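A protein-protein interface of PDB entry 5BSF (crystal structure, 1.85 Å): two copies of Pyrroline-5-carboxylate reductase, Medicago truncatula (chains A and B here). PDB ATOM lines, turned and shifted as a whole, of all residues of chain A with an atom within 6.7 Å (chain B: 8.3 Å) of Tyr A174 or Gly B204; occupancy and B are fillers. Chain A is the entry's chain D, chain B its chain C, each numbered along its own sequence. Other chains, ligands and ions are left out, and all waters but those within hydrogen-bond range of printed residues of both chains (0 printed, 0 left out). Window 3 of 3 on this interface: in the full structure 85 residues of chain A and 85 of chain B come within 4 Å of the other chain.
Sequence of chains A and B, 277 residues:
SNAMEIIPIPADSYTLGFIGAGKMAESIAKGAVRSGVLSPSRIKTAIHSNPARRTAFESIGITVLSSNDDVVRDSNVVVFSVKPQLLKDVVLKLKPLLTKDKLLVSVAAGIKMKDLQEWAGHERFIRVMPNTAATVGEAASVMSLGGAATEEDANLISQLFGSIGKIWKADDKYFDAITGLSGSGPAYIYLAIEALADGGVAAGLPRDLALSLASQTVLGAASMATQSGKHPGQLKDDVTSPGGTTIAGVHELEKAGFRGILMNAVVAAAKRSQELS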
ATOM      1  N   LYS A 169      -1.048  -4.750   6.479  1.00  0.00           N
ATOM      2  CA  LYS A 169       0.277  -4.572   5.864  1.00  0.00           C
ATOM      3  C   LYS A 169       0.383  -5.453   4.666  1.00  0.00           C
ATOM      4  O   LYS A 169      -0.072  -6.551   4.699  1.00  0.00           O
ATOM      5  CB  LYS A 169       1.386  -4.958   6.836  1.00  0.00           C
ATOM      6  CG  LYS A 169       1.392  -4.004   7.994  1.00  0.00           C
ATOM      7  CD  LYS A 169       2.508  -4.217   8.999  1.00  0.00           C
ATOM      8  CE  LYS A 169       2.156  -3.419  10.246  1.00  0.00           C
ATOM      9  NZ  LYS A 169       3.176  -3.690  11.270  1.00  0.00           N
ATOM     10  N   ALA A 170       0.993  -4.967   3.610  1.00  0.00           N
ATOM     11  CA  ALA A 170       1.246  -5.824   2.448  1.00  0.00           C
ATOM     12  C   ALA A 170       2.385  -5.279   1.615  1.00  0.00           C
ATOM     13  O   ALA A 170       2.732  -4.103   1.656  1.00  0.00           O
ATOM     14  CB  ALA A 170       0.016  -5.932   1.589  1.00  0.00           C
ATOM     15  N   ASP A 171       2.990  -6.181   0.879  1.00  0.00           N
ATOM     16  CA  ASP A 171       4.088  -5.872  -0.009  1.00  0.00           C
ATOM     17  C   ASP A 171       3.559  -4.952  -1.111  1.00  0.00           C
ATOM     18  O   ASP A 171       2.405  -5.075  -1.559  1.00  0.00           O
ATOM     19  CB  ASP A 171       4.609  -7.198  -0.529  1.00  0.00           C
ATOM     20  CG  ASP A 171       5.837  -7.093  -1.410  1.00  0.00           C
ATOM     21  OD1 ASP A 171       5.889  -6.262  -2.324  1.00  0.00           O
ATOM     22  OD2 ASP A 171       6.765  -7.924  -1.180  1.00  0.00           O
ATOM     23  N   ASP A 172       4.401  -4.026  -1.530  1.00  0.00           N
ATOM     24  CA  ASP A 172       4.052  -3.030  -2.511  1.00  0.00           C
ATOM     25  C   ASP A 172       3.609  -3.679  -3.802  1.00  0.00           C
ATOM     26  O   ASP A 172       2.743  -3.135  -4.507  1.00  0.00           O
ATOM     27  CB  ASP A 172       5.272  -2.081  -2.760  1.00  0.00           C
ATOM     28  CG  ASP A 172       4.842  -0.665  -3.233  1.00  0.00           C
ATOM     29  OD1 ASP A 172       4.081   0.014  -2.520  1.00  0.00           O
ATOM     30  OD2 ASP A 172       5.160  -0.286  -4.371  1.00  0.00           O
ATOM     31  N   LYS A 173       4.085  -4.879  -4.105  1.00  0.00           N
ATOM     32  CA  LYS A 173       3.693  -5.490  -5.368  1.00  0.00           C
ATOM     33  C   LYS A 173       2.151  -5.884  -5.448  1.00  0.00           C
ATOM     34  O   LYS A 173       1.643  -6.103  -6.515  1.00  0.00           O
ATOM     35  CB  LYS A 173       4.450  -6.733  -5.656  1.00  0.00           C
ATOM     36  CG  LYS A 173       4.074  -7.869  -4.776  1.00  0.00           C
ATOM     37  CD  LYS A 173       4.961  -9.056  -5.049  1.00  0.00           C
ATOM     38  CE  LYS A 173       4.801 -10.034  -3.915  1.00  0.00           C
ATOM     39  NZ  LYS A 173       5.437 -11.309  -4.291  1.00  0.00           N
ATOM     40  N   TYR A 174       1.491  -5.925  -4.314  1.00  0.00           N
ATOM     41  CA  TYR A 174       0.031  -6.239  -4.254  1.00  0.00           C
ATOM     42  C   TYR A 174      -0.877  -5.020  -4.449  1.00  0.00           C
ATOM     43  O   TYR A 174      -2.099  -5.158  -4.498  1.00  0.00           O
ATOM     44  CB  TYR A 174      -0.273  -6.853  -2.919  1.00  0.00           C
ATOM     45  CG  TYR A 174       0.394  -8.191  -2.676  1.00  0.00           C
ATOM     46  CD1 TYR A 174       0.248  -9.212  -3.537  1.00  0.00           C
ATOM     47  CD2 TYR A 174       1.148  -8.424  -1.516  1.00  0.00           C
ATOM     48  CE1 TYR A 174       0.861 -10.436  -3.321  1.00  0.00           C
ATOM     49  CE2 TYR A 174       1.774  -9.641  -1.285  1.00  0.00           C
ATOM     50  CZ  TYR A 174       1.627 -10.627  -2.208  1.00  0.00           C
ATOM     51  OH  TYR A 174       2.209 -11.824  -2.028  1.00  0.00           O
ATOM     52  N   PHE A 175      -0.311  -3.829  -4.548  1.00  0.00           N
ATOM     53  CA  PHE A 175      -1.120  -2.592  -4.546  1.00  0.00           C
ATOM     54  C   PHE A 175      -2.059  -2.357  -5.739  1.00  0.00           C
ATOM     55  O   PHE A 175      -3.137  -1.800  -5.595  1.00  0.00           O
ATOM     56  CB  PHE A 175      -0.284  -1.363  -4.164  1.00  0.00           C
ATOM     57  CG  PHE A 175      -0.113  -1.186  -2.644  1.00  0.00           C
ATOM     58  CD1 PHE A 175       0.526  -2.173  -1.885  1.00  0.00           C
ATOM     59  CD2 PHE A 175      -0.613  -0.143  -1.991  1.00  0.00           C
ATOM     60  CE1 PHE A 175       0.636  -2.064  -0.523  1.00  0.00           C
ATOM     61  CE2 PHE A 175      -0.427   0.025  -0.631  1.00  0.00           C
ATOM     62  CZ  PHE A 175       0.181  -0.956   0.111  1.00  0.00           C
ATOM     63  N   ASP A 176      -1.712  -2.826  -6.918  1.00  0.00           N
ATOM     64  CA  ASP A 176      -2.722  -2.821  -8.014  1.00  0.00           C
ATOM     65  C   ASP A 176      -3.956  -3.615  -7.740  1.00  0.00           C
ATOM     66  O   ASP A 176      -5.070  -3.179  -7.988  1.00  0.00           O
ATOM     67  CB  ASP A 176      -2.099  -3.343  -9.310  1.00  0.00           C
ATOM     68  CG  ASP A 176      -1.121  -2.358  -9.908  1.00  0.00           C
ATOM     69  OD1 ASP A 176      -1.332  -1.134  -9.820  1.00  0.00           O
ATOM     70  OD2 ASP A 176      -0.115  -2.825 -10.436  1.00  0.00           O
ATOM     71  N   ALA A 177      -3.768  -4.869  -7.307  1.00  0.00           N
ATOM     72  CA  ALA A 177      -4.880  -5.699  -6.928  1.00  0.00           C
ATOM     73  C   ALA A 177      -5.659  -5.082  -5.738  1.00  0.00           C
ATOM     74  O   ALA A 177      -6.918  -5.132  -5.673  1.00  0.00           O
ATOM     75  CB  ALA A 177      -4.454  -7.106  -6.580  1.00  0.00           C
ATOM     76  N   ILE A 178      -4.933  -4.584  -4.736  1.00  0.00           N
ATOM     77  CA  ILE A 178      -5.629  -3.913  -3.595  1.00  0.00           C
ATOM     78  C   ILE A 178      -6.549  -2.816  -4.169  1.00  0.00           C
ATOM     79  O   ILE A 178      -7.721  -2.644  -3.772  1.00  0.00           O
ATOM     80  CB  ILE A 178      -4.628  -3.389  -2.586  1.00  0.00           C
ATOM     81  CG1 ILE A 178      -3.992  -4.593  -1.860  1.00  0.00           C
ATOM     82  CG2 ILE A 178      -5.277  -2.440  -1.571  1.00  0.00           C
ATOM     83  CD1 ILE A 178      -2.693  -4.265  -1.107  1.00  0.00           C
ATOM     84  N   THR A 179      -5.990  -2.057  -5.065  1.00  0.00           N
ATOM     85  CA  THR A 179      -6.711  -0.863  -5.664  1.00  0.00           C
ATOM     86  C   THR A 179      -8.013  -1.363  -6.310  1.00  0.00           C
ATOM     87  O   THR A 179      -9.042  -0.756  -6.159  1.00  0.00           O
ATOM     88  CB  THR A 179      -5.836  -0.119  -6.667  1.00  0.00           C
ATOM     89  OG1 THR A 179      -4.660   0.377  -5.962  1.00  0.00           O
ATOM     90  CG2 THR A 179      -6.536   1.044  -7.277  1.00  0.00           C
ATOM     91  N   ALA B 197     -13.426 -11.467  -2.408  1.00  0.00           N
ATOM     92  CA  ALA B 197     -12.199 -12.106  -1.958  1.00  0.00           C
ATOM     93  C   ALA B 197     -11.579 -13.030  -2.998  1.00  0.00           C
ATOM     94  O   ALA B 197     -10.375 -12.932  -3.290  1.00  0.00           O
ATOM     95  CB  ALA B 197     -12.451 -12.902  -0.674  1.00  0.00           C
ATOM     96  N   ASP B 198     -12.409 -13.860  -3.631  1.00  0.00           N
ATOM     97  CA  ASP B 198     -11.940 -14.668  -4.709  1.00  0.00           C
ATOM     98  C   ASP B 198     -11.350 -13.854  -5.862  1.00  0.00           C
ATOM     99  O   ASP B 198     -10.347 -14.219  -6.472  1.00  0.00           O
ATOM    100  CB  ASP B 198     -13.077 -15.580  -5.242  1.00  0.00           C
ATOM    101  CG  ASP B 198     -13.419 -16.768  -4.311  1.00  0.00           C
ATOM    102  OD1 ASP B 198     -12.564 -17.234  -3.497  1.00  0.00           O
ATOM    103  OD2 ASP B 198     -14.592 -17.274  -4.438  1.00  0.00           O
ATOM    104  N   GLY B 199     -12.003 -12.718  -6.163  1.00  0.00           N
ATOM    105  CA  GLY B 199     -11.509 -11.792  -7.176  1.00  0.00           C
ATOM    106  C   GLY B 199     -10.136 -11.256  -6.823  1.00  0.00           C
ATOM    107  O   GLY B 199      -9.257 -11.200  -7.609  1.00  0.00           O
ATOM    108  N   GLY B 200     -10.009 -10.868  -5.566  1.00  0.00           N
ATOM    109  CA  GLY B 200      -8.714 -10.413  -5.081  1.00  0.00           C
ATOM    110  C   GLY B 200      -7.634 -11.457  -5.284  1.00  0.00           C
ATOM    111  O   GLY B 200      -6.534 -11.139  -5.757  1.00  0.00           O
ATOM    112  N   VAL B 201      -7.898 -12.660  -4.827  1.00  0.00           N
ATOM    113  CA  VAL B 201      -6.958 -13.816  -5.005  1.00  0.00           C
ATOM    114  C   VAL B 201      -6.678 -13.992  -6.473  1.00  0.00           C
ATOM    115  O   VAL B 201      -5.520 -14.205  -6.917  1.00  0.00           O
ATOM    116  CB  VAL B 201      -7.498 -15.058  -4.318  1.00  0.00           C
ATOM    117  CG1 VAL B 201      -6.636 -16.266  -4.595  1.00  0.00           C
ATOM    118  CG2 VAL B 201      -7.523 -14.840  -2.811  1.00  0.00           C
ATOM    119  N   ALA B 202      -7.703 -13.933  -7.300  1.00  0.00           N
ATOM    120  CA  ALA B 202      -7.495 -14.077  -8.757  1.00  0.00           C
ATOM    121  C   ALA B 202      -6.546 -12.994  -9.329  1.00  0.00           C
ATOM    122  O   ALA B 202      -5.857 -13.232 -10.316  1.00  0.00           O
ATOM    123  CB  ALA B 202      -8.801 -14.072  -9.504  1.00  0.00           C
ATOM    124  N   ALA B 203      -6.578 -11.799  -8.731  1.00  0.00           N
ATOM    125  CA  ALA B 203      -5.718 -10.695  -9.099  1.00  0.00           C
ATOM    126  C   ALA B 203      -4.390 -10.721  -8.415  1.00  0.00           C
ATOM    127  O   ALA B 203      -3.608  -9.791  -8.547  1.00  0.00           O
ATOM    128  CB  ALA B 203      -6.431  -9.379  -8.799  1.00  0.00           C
ATOM    129  N   GLY B 204      -4.120 -11.724  -7.621  1.00  0.00           N
ATOM    130  CA  GLY B 204      -2.776 -11.941  -6.983  1.00  0.00           C
ATOM    131  C   GLY B 204      -2.666 -11.711  -5.515  1.00  0.00           C
ATOM    132  O   GLY B 204      -1.573 -11.827  -4.954  1.00  0.00           O
ATOM    133  N   LEU B 205      -3.772 -11.392  -4.828  1.00  0.00           N
ATOM    134  CA  LEU B 205      -3.707 -11.154  -3.402  1.00  0.00           C
ATOM    135  C   LEU B 205      -3.621 -12.414  -2.553  1.00  0.00           C
ATOM    136  O   LEU B 205      -4.298 -13.393  -2.835  1.00  0.00           O
ATOM    137  CB  LEU B 205      -4.870 -10.334  -2.892  1.00  0.00           C
ATOM    138  CG  LEU B 205      -5.047  -8.956  -3.463  1.00  0.00           C
ATOM    139  CD1 LEU B 205      -6.263  -8.290  -2.799  1.00  0.00           C
ATOM    140  CD2 LEU B 205      -3.782  -8.131  -3.212  1.00  0.00           C
ATOM    141  N   PRO B 206      -2.910 -12.341  -1.436  1.00  0.00           N
ATOM    142  CA  PRO B 206      -3.053 -13.402  -0.448  1.00  0.00           C
ATOM    143  C   PRO B 206      -4.535 -13.484  -0.007  1.00  0.00           C
ATOM    144  O   PRO B 206      -5.227 -12.480   0.184  1.00  0.00           O
ATOM    145  CB  PRO B 206      -2.216 -12.921   0.775  1.00  0.00           C
ATOM    146  CG  PRO B 206      -1.172 -11.985   0.144  1.00  0.00           C
ATOM    147  CD  PRO B 206      -2.008 -11.273  -0.960  1.00  0.00           C
ATOM    148  N   ARG B 207      -4.936 -14.681   0.318  1.00  0.00           N
ATOM    149  CA  ARG B 207      -6.357 -14.953   0.736  1.00  0.00           C
ATOM    150  C   ARG B 207      -6.780 -14.200   2.002  1.00  0.00           C
ATOM    151  O   ARG B 207      -7.849 -13.646   2.053  1.00  0.00           O
ATOM    152  CB  ARG B 207      -6.510 -16.473   0.929  1.00  0.00           C
ATOM    153  CG  ARG B 207      -7.822 -16.913   1.564  1.00  0.00           C
ATOM    154  CD  ARG B 207      -9.043 -16.594   0.716  1.00  0.00           C
ATOM    155  NE  ARG B 207      -9.069 -17.326  -0.535  1.00  0.00           N
ATOM    156  CZ  ARG B 207     -10.009 -17.191  -1.482  1.00  0.00           C
ATOM    157  NH1 ARG B 207     -11.046 -16.387  -1.300  1.00  0.00           N
ATOM    158  NH2 ARG B 207      -9.885 -17.842  -2.621  1.00  0.00           N
ATOM    159  N   LEU B 209      -5.675 -11.479   3.393  1.00  0.00           N
ATOM    160  CA  LEU B 209      -5.802 -10.036   3.123  1.00  0.00           C
ATOM    161  C   LEU B 209      -7.018  -9.790   2.211  1.00  0.00           C
ATOM    162  O   LEU B 209      -7.764  -8.844   2.429  1.00  0.00           O
ATOM    163  CB  LEU B 209      -4.566  -9.512   2.410  1.00  0.00           C
ATOM    164  CG  LEU B 209      -4.606  -8.036   2.004  1.00  0.00           C
ATOM    165  CD1 LEU B 209      -4.639  -7.178   3.272  1.00  0.00           C
ATOM    166  CD2 LEU B 209      -3.361  -7.663   1.200  1.00  0.00           C
ATOM    167  N   ALA B 210      -7.193 -10.647   1.223  1.00  0.00           N
ATOM    168  CA  ALA B 210      -8.344 -10.460   0.263  1.00  0.00           C
ATOM    169  C   ALA B 210      -9.677 -10.516   0.982  1.00  0.00           C
ATOM    170  O   ALA B 210     -10.547  -9.679   0.789  1.00  0.00           O
ATOM    171  CB  ALA B 210      -8.289 -11.458  -0.848  1.00  0.00           C
ATOM    172  N   LEU B 213      -9.992  -7.432   3.390  1.00  0.00           N
ATOM    173  CA  LEU B 213     -10.321  -6.226   2.580  1.00  0.00           C
ATOM    174  C   LEU B 213     -11.731  -6.266   2.053  1.00  0.00           C
ATOM    175  O   LEU B 213     -12.460  -5.265   2.065  1.00  0.00           O
ATOM    176  CB  LEU B 213      -9.356  -6.021   1.422  1.00  0.00           C
ATOM    177  CG  LEU B 213      -7.905  -5.670   1.814  1.00  0.00           C
ATOM    178  CD1 LEU B 213      -7.045  -5.616   0.561  1.00  0.00           C
ATOM    179  CD2 LEU B 213      -7.840  -4.347   2.527  1.00  0.00           C
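The backbone carbonyl oxygen of Gly B200 lies within hydrogen-bond range of the backbone NH of Leu B205 (2.9 Å).
Among the printed residues, pairs that only touch across the chains: Ala A170 with Leu B209, Tyr A174 with Gly B204, Tyr A174 with Leu B205, Tyr A174 with Pro B206, Ala A177 with Ala B203, Ala A177 with Leu B205 and Ile A178 with Leu B205.
Lys A169 touches none of the printed residues of chain B. Of the printed residues of chain B, Ala A170 touches Leu B209 (3.8 Å). Of chain B, only Gly B204, Leu B205 and Pro B206 come within 4 Å of Tyr A174. Of the printed residues of chain B, Ala A177 touches Ala B203 and Leu B205. Printed residues of chain A within 4 Å of Gly B204: Tyr A174 (3.2 Å). The nearest residue of chain B that does not touch Tyr A174 is Leu B209 (5.2 Å). The nearest residue of chain A that does not touch Gly B204 is Ala A177 (4.7 Å).
Of the 11 printed residues of chain A, 4 touch a printed residue of chain B. Hydrophobic or aromatic side chains of chain B within 4 Å of the printed part of chain A: Ala B203, Leu B205, Pro B206 and Leu B209. Among the printed residues, no Asp or Glu carboxylate lies within 4 Å of a Lys or Arg side-chain nitrogen of the other chain.
No position is printed for both chains. Of the 7 pairs that touch across the chains among the printed residues, none has its exchanged pair printed and touching as well.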
